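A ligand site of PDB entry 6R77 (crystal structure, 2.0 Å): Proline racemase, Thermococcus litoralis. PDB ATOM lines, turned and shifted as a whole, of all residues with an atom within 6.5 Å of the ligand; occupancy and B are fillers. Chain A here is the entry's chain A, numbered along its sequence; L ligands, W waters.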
ATOM      1  N   GLU A  50     -32.969  21.417  17.178  1.00  0.00           N
ATOM      2  CA  GLU A  50     -32.290  22.182  16.102  1.00  0.00           C
ATOM      3  C   GLU A  50     -33.323  22.677  15.088  1.00  0.00           C
ATOM      4  O   GLU A  50     -34.081  21.910  14.505  1.00  0.00           O
ATOM      5  CB  GLU A  50     -31.215  21.343  15.424  1.00  0.00           C
ATOM      6  CG  GLU A  50     -30.431  22.106  14.370  1.00  0.00           C
ATOM      7  CD  GLU A  50     -29.430  23.134  14.862  1.00  0.00           C
ATOM      8  OE1 GLU A  50     -29.342  23.326  16.098  1.00  0.00           O
ATOM      9  OE2 GLU A  50     -28.730  23.726  14.001  1.00  0.00           O
ATOM     10  N   TYR A  96     -31.326  27.901  11.217  1.00  0.00           N
ATOM     11  CA  TYR A  96     -30.947  27.048  10.058  1.00  0.00           C
ATOM     12  C   TYR A  96     -32.140  27.017   9.111  1.00  0.00           C
ATOM     13  O   TYR A  96     -33.249  27.021   9.624  1.00  0.00           O
ATOM     14  CB  TYR A  96     -30.492  25.666  10.557  1.00  0.00           C
ATOM     15  CG  TYR A  96     -29.632  24.902   9.600  1.00  0.00           C
ATOM     16  CD1 TYR A  96     -30.175  24.200   8.527  1.00  0.00           C
ATOM     17  CD2 TYR A  96     -28.255  24.891   9.744  1.00  0.00           C
ATOM     18  CE1 TYR A  96     -29.364  23.476   7.652  1.00  0.00           C
ATOM     19  CE2 TYR A  96     -27.434  24.174   8.888  1.00  0.00           C
ATOM     20  CZ  TYR A  96     -27.994  23.475   7.829  1.00  0.00           C
ATOM     21  OH  TYR A  96     -27.151  22.826   6.970  1.00  0.00           O
ATOM     22  N   HIS A 116     -27.474  28.786   6.809  1.00  0.00           N
ATOM     23  CA  HIS A 116     -27.117  28.973   8.235  1.00  0.00           C
ATOM     24  C   HIS A 116     -26.590  30.380   8.460  1.00  0.00           C
ATOM     25  O   HIS A 116     -26.846  31.247   7.610  1.00  0.00           O
ATOM     26  CB  HIS A 116     -26.173  27.847   8.685  1.00  0.00           C
ATOM     27  CG  HIS A 116     -24.955  27.655   7.851  1.00  0.00           C
ATOM     28  ND1 HIS A 116     -24.235  28.695   7.329  1.00  0.00           N
ATOM     29  CD2 HIS A 116     -24.287  26.513   7.543  1.00  0.00           C
ATOM     30  CE1 HIS A 116     -23.184  28.222   6.690  1.00  0.00           C
ATOM     31  NE2 HIS A 116     -23.191  26.872   6.821  1.00  0.00           N
ATOM     32  N   SER A 121     -25.668  26.302   2.417  1.00  0.00           N
ATOM     33  CA  SER A 121     -24.935  25.149   3.007  1.00  0.00           C
ATOM     34  C   SER A 121     -25.145  23.885   2.168  1.00  0.00           C
ATOM     35  O   SER A 121     -26.175  23.770   1.436  1.00  0.00           O
ATOM     36  CB  SER A 121     -25.409  24.915   4.426  1.00  0.00           C
ATOM     37  OG  SER A 121     -24.907  23.696   4.973  1.00  0.00           O
ATOM     38  N   THR A 122     -24.220  22.951   2.341  1.00  0.00           N
ATOM     39  CA  THR A 122     -24.321  21.564   1.840  1.00  0.00           C
ATOM     40  C   THR A 122     -25.250  20.778   2.758  1.00  0.00           C
ATOM     41  O   THR A 122     -25.915  21.381   3.651  1.00  0.00           O
ATOM     42  CB  THR A 122     -22.938  20.930   1.642  1.00  0.00           C
ATOM     43  OG1 THR A 122     -23.149  19.707   0.938  1.00  0.00           O
ATOM     44  CG2 THR A 122     -22.202  20.689   2.940  1.00  0.00           C
ATOM     45  N   MET A 123     -25.281  19.463   2.533  1.00  0.00           N
ATOM     46  CA  MET A 123     -26.189  18.493   3.172  1.00  0.00           C
ATOM     47  C   MET A 123     -26.242  18.675   4.700  1.00  0.00           C
ATOM     48  O   MET A 123     -25.232  19.009   5.301  1.00  0.00           O
ATOM     49  CB  MET A 123     -25.713  17.084   2.803  1.00  0.00           C
ATOM     50  CG  MET A 123     -26.374  15.995   3.574  1.00  0.00           C
ATOM     51  SD  MET A 123     -28.125  15.957   3.295  1.00  0.00           S
ATOM     52  CE  MET A 123     -28.519  14.588   4.380  1.00  0.00           C
ATOM     53  N   CYS A 124     -27.401  18.390   5.295  1.00  0.00           N
ATOM     54  CA  CYS A 124     -27.642  18.501   6.748  1.00  0.00           C
ATOM     55  C   CYS A 124     -28.697  17.475   7.156  1.00  0.00           C
ATOM     56  O   CYS A 124     -29.751  17.443   6.547  1.00  0.00           O
ATOM     57  CB  CYS A 124     -28.093  19.923   7.087  1.00  0.00           C
ATOM     58  SG  CYS A 124     -28.849  20.060   8.728  1.00  0.00           S
ATOM     59  N   GLY A 125     -28.381  16.662   8.162  1.00  0.00           N
ATOM     60  CA  GLY A 125     -29.211  15.516   8.593  1.00  0.00           C
ATOM     61  C   GLY A 125     -30.425  15.942   9.395  1.00  0.00           C
ATOM     62  O   GLY A 125     -31.511  15.365   9.182  1.00  0.00           O
ATOM     63  N   HIS A 126     -30.278  16.893  10.319  1.00  0.00           N
ATOM     64  CA  HIS A 126     -31.420  17.306  11.165  1.00  0.00           C
ATOM     65  C   HIS A 126     -32.489  17.866  10.229  1.00  0.00           C
ATOM     66  O   HIS A 126     -33.680  17.614  10.438  1.00  0.00           O
ATOM     67  CB  HIS A 126     -31.015  18.280  12.281  1.00  0.00           C
ATOM     68  CG  HIS A 126     -31.198  19.703  11.891  1.00  0.00           C
ATOM     69  ND1 HIS A 126     -30.163  20.456  11.431  1.00  0.00           N
ATOM     70  CD2 HIS A 126     -32.294  20.478  11.863  1.00  0.00           C
ATOM     71  CE1 HIS A 126     -30.600  21.662  11.123  1.00  0.00           C
ATOM     72  NE2 HIS A 126     -31.915  21.698  11.367  1.00  0.00           N
ATOM     73  N   ALA A 127     -32.065  18.575   9.193  1.00  0.00           N
ATOM     74  CA  ALA A 127     -32.996  19.224   8.248  1.00  0.00           C
ATOM     75  C   ALA A 127     -33.701  18.161   7.389  1.00  0.00           C
ATOM     76  O   ALA A 127     -34.926  18.271   7.151  1.00  0.00           O
ATOM     77  CB  ALA A 127     -32.236  20.233   7.412  1.00  0.00           C
ATOM     78  N   PHE A 175     -32.912   8.532   7.299  1.00  0.00           N
ATOM     79  CA  PHE A 175     -32.339   8.742   5.940  1.00  0.00           C
ATOM     80  C   PHE A 175     -31.109   7.860   5.807  1.00  0.00           C
ATOM     81  O   PHE A 175     -30.482   7.510   6.824  1.00  0.00           O
ATOM     82  CB  PHE A 175     -32.107  10.222   5.654  1.00  0.00           C
ATOM     83  CG  PHE A 175     -31.023  10.877   6.453  1.00  0.00           C
ATOM     84  CD1 PHE A 175     -31.307  11.483   7.669  1.00  0.00           C
ATOM     85  CD2 PHE A 175     -29.716  10.915   5.976  1.00  0.00           C
ATOM     86  CE1 PHE A 175     -30.317  12.124   8.396  1.00  0.00           C
ATOM     87  CE2 PHE A 175     -28.705  11.533   6.721  1.00  0.00           C
ATOM     88  CZ  PHE A 175     -29.015  12.126   7.929  1.00  0.00           C
ATOM     89  N   GLY A 204     -19.389  12.881   6.196  1.00  0.00           N
ATOM     90  CA  GLY A 204     -20.748  12.320   6.355  1.00  0.00           C
ATOM     91  C   GLY A 204     -21.752  13.149   5.575  1.00  0.00           C
ATOM     92  O   GLY A 204     -22.837  13.385   6.104  1.00  0.00           O
ATOM     93  N   ALA A 206     -20.769  16.119   4.935  1.00  0.00           N
ATOM     94  CA  ALA A 206     -19.938  17.304   5.243  1.00  0.00           C
ATOM     95  C   ALA A 206     -18.687  16.794   5.952  1.00  0.00           C
ATOM     96  O   ALA A 206     -18.740  15.661   6.475  1.00  0.00           O
ATOM     97  CB  ALA A 206     -20.710  18.282   6.076  1.00  0.00           C
ATOM     98  N   TYR A 208     -15.946  16.877   8.989  1.00  0.00           N
ATOM     99  CA  TYR A 208     -15.806  17.249  10.423  1.00  0.00           C
ATOM    100  C   TYR A 208     -14.473  16.766  10.988  1.00  0.00           C
ATOM    101  O   TYR A 208     -14.038  15.641  10.642  1.00  0.00           O
ATOM    102  CB  TYR A 208     -16.934  16.661  11.250  1.00  0.00           C
ATOM    103  CG  TYR A 208     -18.265  17.223  10.903  1.00  0.00           C
ATOM    104  CD1 TYR A 208     -18.631  18.492  11.300  1.00  0.00           C
ATOM    105  CD2 TYR A 208     -19.151  16.481  10.142  1.00  0.00           C
ATOM    106  CE1 TYR A 208     -19.853  19.026  10.929  1.00  0.00           C
ATOM    107  CE2 TYR A 208     -20.389  16.986   9.788  1.00  0.00           C
ATOM    108  CZ  TYR A 208     -20.739  18.261  10.175  1.00  0.00           C
ATOM    109  OH  TYR A 208     -21.974  18.719   9.836  1.00  0.00           O
ATOM    110  N   TYR A 257     -16.486  21.719   7.366  1.00  0.00           N
ATOM    111  CA  TYR A 257     -17.774  22.245   7.851  1.00  0.00           C
ATOM    112  C   TYR A 257     -17.665  22.617   9.334  1.00  0.00           C
ATOM    113  O   TYR A 257     -18.260  23.607   9.721  1.00  0.00           O
ATOM    114  CB  TYR A 257     -18.875  21.213   7.623  1.00  0.00           C
ATOM    115  CG  TYR A 257     -20.282  21.749   7.617  1.00  0.00           C
ATOM    116  CD1 TYR A 257     -20.868  22.236   6.457  1.00  0.00           C
ATOM    117  CD2 TYR A 257     -21.046  21.734   8.765  1.00  0.00           C
ATOM    118  CE1 TYR A 257     -22.156  22.737   6.457  1.00  0.00           C
ATOM    119  CE2 TYR A 257     -22.343  22.217   8.781  1.00  0.00           C
ATOM    120  CZ  TYR A 257     -22.910  22.728   7.624  1.00  0.00           C
ATOM    121  OH  TYR A 257     -24.202  23.182   7.668  1.00  0.00           O
ATOM    122  N   CYS A 276     -21.473  19.881  17.817  1.00  0.00           N
ATOM    123  CA  CYS A 276     -20.957  20.331  16.509  1.00  0.00           C
ATOM    124  C   CYS A 276     -20.890  21.866  16.497  1.00  0.00           C
ATOM    125  O   CYS A 276     -21.942  22.487  16.673  1.00  0.00           O
ATOM    126  CB  CYS A 276     -21.841  19.826  15.377  1.00  0.00           C
ATOM    127  SG  CYS A 276     -21.312  20.480  13.771  1.00  0.00           S
ATOM    128  N   PHE A 278     -20.044  24.779  13.875  1.00  0.00           N
ATOM    129  CA  PHE A 278     -20.053  24.874  12.410  1.00  0.00           C
ATOM    130  C   PHE A 278     -20.328  26.322  12.030  1.00  0.00           C
ATOM    131  O   PHE A 278     -20.646  27.142  12.922  1.00  0.00           O
ATOM    132  CB  PHE A 278     -21.068  23.904  11.801  1.00  0.00           C
ATOM    133  CG  PHE A 278     -22.527  24.237  12.035  1.00  0.00           C
ATOM    134  CD1 PHE A 278     -23.151  23.901  13.230  1.00  0.00           C
ATOM    135  CD2 PHE A 278     -23.276  24.902  11.070  1.00  0.00           C
ATOM    136  CE1 PHE A 278     -24.494  24.210  13.435  1.00  0.00           C
ATOM    137  CE2 PHE A 278     -24.607  25.221  11.281  1.00  0.00           C
ATOM    138  CZ  PHE A 278     -25.221  24.879  12.467  1.00  0.00           C
ATOM    139  N   VAL A 283     -23.818  26.518  16.797  1.00  0.00           N
ATOM    140  CA  VAL A 283     -23.821  25.265  17.589  1.00  0.00           C
ATOM    141  C   VAL A 283     -25.086  24.474  17.252  1.00  0.00           C
ATOM    142  O   VAL A 283     -26.201  25.016  17.346  1.00  0.00           O
ATOM    143  CB  VAL A 283     -23.692  25.522  19.110  1.00  0.00           C
ATOM    144  CG1 VAL A 283     -23.631  24.218  19.894  1.00  0.00           C
ATOM    145  CG2 VAL A 283     -22.500  26.411  19.432  1.00  0.00           C
ATOM    146  N   ASP A 284     -24.894  23.206  16.897  1.00  0.00           N
ATOM    147  CA  ASP A 284     -26.017  22.286  16.605  1.00  0.00           C
ATOM    148  C   ASP A 284     -26.559  21.808  17.953  1.00  0.00           C
ATOM    149  O   ASP A 284     -25.775  21.247  18.747  1.00  0.00           O
ATOM    150  CB  ASP A 284     -25.539  21.147  15.695  1.00  0.00           C
ATOM    151  CG  ASP A 284     -26.643  20.330  15.057  1.00  0.00           C
ATOM    152  OD1 ASP A 284     -27.832  20.540  15.418  1.00  0.00           O
ATOM    153  OD2 ASP A 284     -26.305  19.457  14.240  1.00  0.00           O
ATOM    154  N   ARG A 285     -27.855  21.996  18.161  1.00  0.00           N
ATOM    155  CA  ARG A 285     -28.587  21.487  19.341  1.00  0.00           C
ATOM    156  C   ARG A 285     -28.944  20.006  19.138  1.00  0.00           C
ATOM    157  O   ARG A 285     -29.349  19.363  20.109  1.00  0.00           O
ATOM    158  CB  ARG A 285     -29.852  22.309  19.576  1.00  0.00           C
ATOM    159  CG  ARG A 285     -29.614  23.720  20.106  1.00  0.00           C
ATOM    160  CD  ARG A 285     -29.186  24.776  19.085  1.00  0.00           C
ATOM    161  NE  ARG A 285     -29.256  26.100  19.728  1.00  0.00           N
ATOM    162  CZ  ARG A 285     -28.222  26.874  20.031  1.00  0.00           C
ATOM    163  NH1 ARG A 285     -26.985  26.542  19.711  1.00  0.00           N
ATOM    164  NH2 ARG A 285     -28.449  28.023  20.642  1.00  0.00           N
ATOM    165  N   SER A 286     -28.878  19.509  17.903  1.00  0.00           N
ATOM    166  CA  SER A 286     -29.069  18.076  17.599  1.00  0.00           C
ATOM    167  C   SER A 286     -27.724  17.390  17.710  1.00  0.00           C
ATOM    168  O   SER A 286     -26.690  18.039  17.773  1.00  0.00           O
ATOM    169  CB  SER A 286     -29.692  17.864  16.215  1.00  0.00           C
ATOM    170  OG  SER A 286     -28.725  17.964  15.172  1.00  0.00           O
ATOM    171  N   PRO A 287     -27.698  16.024  17.673  1.00  0.00           N
ATOM    172  CA  PRO A 287     -26.440  15.297  17.537  1.00  0.00           C
ATOM    173  C   PRO A 287     -25.716  15.483  16.200  1.00  0.00           C
ATOM    174  O   PRO A 287     -24.591  14.999  16.098  1.00  0.00           O
ATOM    175  CB  PRO A 287     -26.864  13.839  17.756  1.00  0.00           C
ATOM    176  CG  PRO A 287     -28.170  13.916  18.506  1.00  0.00           C
ATOM    177  CD  PRO A 287     -28.841  15.138  17.897  1.00  0.00           C
ATOM    178  N   THR A 288     -26.350  16.167  15.229  1.00  0.00           N
ATOM    179  CA  THR A 288     -25.820  16.433  13.875  1.00  0.00           C
ATOM    180  C   THR A 288     -25.919  15.144  13.037  1.00  0.00           C
ATOM    181  O   THR A 288     -25.174  14.195  13.329  1.00  0.00           O
ATOM    182  CB  THR A 288     -24.379  16.965  13.914  1.00  0.00           C
ATOM    183  OG1 THR A 288     -24.289  17.976  14.919  1.00  0.00           O
ATOM    184  CG2 THR A 288     -23.936  17.574  12.605  1.00  0.00           C
ATOM    185  N   GLY A 289     -26.766  15.108  12.019  1.00  0.00           N
ATOM    186  CA  GLY A 289     -26.983  13.904  11.186  1.00  0.00           C
ATOM    187  C   GLY A 289     -25.792  13.601  10.287  1.00  0.00           C
ATOM    188  O   GLY A 289     -25.427  12.428  10.187  1.00  0.00           O
ATOM    189  N   THR A 290     -25.219  14.604   9.639  1.00  0.00           N
ATOM    190  CA  THR A 290     -23.937  14.468   8.895  1.00  0.00           C
ATOM    191  C   THR A 290     -22.810  14.083   9.848  1.00  0.00           C
ATOM    192  O   THR A 290     -21.860  13.378   9.416  1.00  0.00           O
ATOM    193  CB  THR A 290     -23.594  15.746   8.134  1.00  0.00           C
ATOM    194  OG1 THR A 290     -23.656  16.835   9.052  1.00  0.00           O
ATOM    195  CG2 THR A 290     -24.551  15.944   6.992  1.00  0.00           C
ATOM    196  N   GLY A 291     -22.910  14.513  11.107  1.00  0.00           N
ATOM    197  CA  GLY A 291     -21.940  14.196  12.165  1.00  0.00           C
ATOM    198  C   GLY A 291     -22.003  12.736  12.543  1.00  0.00           C
ATOM    199  O   GLY A 291     -20.941  12.095  12.634  1.00  0.00           O
ATOM    200  N   PHE A 321     -30.213  11.053  18.266  1.00  0.00           N
ATOM    201  CA  PHE A 321     -30.420  10.371  16.972  1.00  0.00           C
ATOM    202  C   PHE A 321     -29.975   8.925  17.137  1.00  0.00           C
ATOM    203  O   PHE A 321     -29.103   8.667  17.989  1.00  0.00           O
ATOM    204  CB  PHE A 321     -29.629  11.039  15.856  1.00  0.00           C
ATOM    205  CG  PHE A 321     -30.097  12.394  15.399  1.00  0.00           C
ATOM    206  CD1 PHE A 321     -31.394  12.831  15.595  1.00  0.00           C
ATOM    207  CD2 PHE A 321     -29.221  13.217  14.705  1.00  0.00           C
ATOM    208  CE1 PHE A 321     -31.802  14.076  15.147  1.00  0.00           C
ATOM    209  CE2 PHE A 321     -29.628  14.463  14.257  1.00  0.00           C
ATOM    210  CZ  PHE A 321     -30.920  14.884  14.471  1.00  0.00           C
HETATM  211  C1  LIG L   1     -26.822  18.130  10.485  1.00  0.00           C
HETATM  212  O1  LIG L   1     -27.629  17.573  11.281  1.00  0.00           O
HETATM  213  N1  LIG L   1     -27.372  20.276  11.799  1.00  0.00           N
HETATM  214  C2  LIG L   1     -26.748  19.640  10.488  1.00  0.00           C
HETATM  215  C3  LIG L   1     -25.502  20.140  10.427  1.00  0.00           C
HETATM  216  C4  LIG L   1     -25.512  21.459  11.250  1.00  0.00           C
HETATM  217  C5  LIG L   1     -26.998  21.536  11.807  1.00  0.00           C
HETATM  218  O2  LIG L   1     -25.311  20.381   9.042  1.00  0.00           O
HETATM  219  O3  LIG L   1     -26.101  17.493   9.656  1.00  0.00           O
HETATM  220  O   HOH W   1     -23.843  19.008   7.612  1.00  0.00           O
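An oxygen (O3) of the ligand lies within hydrogen-bond range of the side-chain hydroxyl (OG1) of Thr 290, at 2.6 Å. O3 of the ligand lies within hydrogen-bond range of N of Gly 125, at 2.8 Å. An oxygen (O2) of the ligand is in hydrogen-bond range of the side-chain hydroxyl (OH) of Tyr 257 (3.3 Å). N1 of the ligand lies within salt-bridge range of OD2 of Asp 284. A ring nitrogen (ND1) of His 126 is in hydrogen-bond range of a nitrogen (N1) of the ligand (2.8 Å). N of Thr 290 is in hydrogen-bond range of O3 of the ligand, 3.0 Å away. SG of Cys 124 lies close to N1 of the ligand (3.4 Å). The backbone NH (N) of His 126 sits at hydrogen-bond distance from an oxygen (O1) of the ligand. N of Gly 289 is in hydrogen-bond range of O1 of the ligand, 2.7 Å away.
The side-chain hydroxyl (OG) of Ser 121 lies within hydrogen-bond range of the side-chain hydroxyl (OH) of Tyr 257. The side-chain sulfur (SG) of Cys 124 sits close to the side-chain hydroxyl (OH) of Tyr 96 (3.7 Å). The side-chain hydroxyl (OG1) of Thr 288 lies within hydrogen-bond range of the side-chain carboxylate (OD2) of Asp 284 (2.6 Å). The side-chain sulfur of Cys 124 lies within hydrogen-bond range of the backbone NH of Ala 127, 3.6 Å away. The backbone NH of Asp 284 sits at hydrogen-bond distance from the backbone carbonyl oxygen of Cys 276, 3.0 Å away. The side-chain carboxylate of Asp 284 lies within hydrogen-bond range of the side-chain hydroxyl of Ser 286, at 2.7 Å. OH of Tyr 96 sits at hydrogen-bond distance from OG of Ser 121 (3.1 Å). The side-chain carboxylate (OE1) of Glu 50 lies within hydrogen-bond range of the backbone NH (N) of Arg 285 (2.9 Å).
Residues that only touch the ligand: Thr 288 (3.4 Å), Glu 50 (3.6 Å), Phe 278 (3.6 Å), Tyr 96 (3.7 Å), Tyr 208 (3.8 Å) and Met 123 (3.99 Å).
Water W1 lies within hydrogen-bond range of O2 of the ligand (2.5 Å), OG1 of Thr 290 (2.6 Å), O of Met 123 (2.7 Å) and OH of Tyr 208 (2.9 Å).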
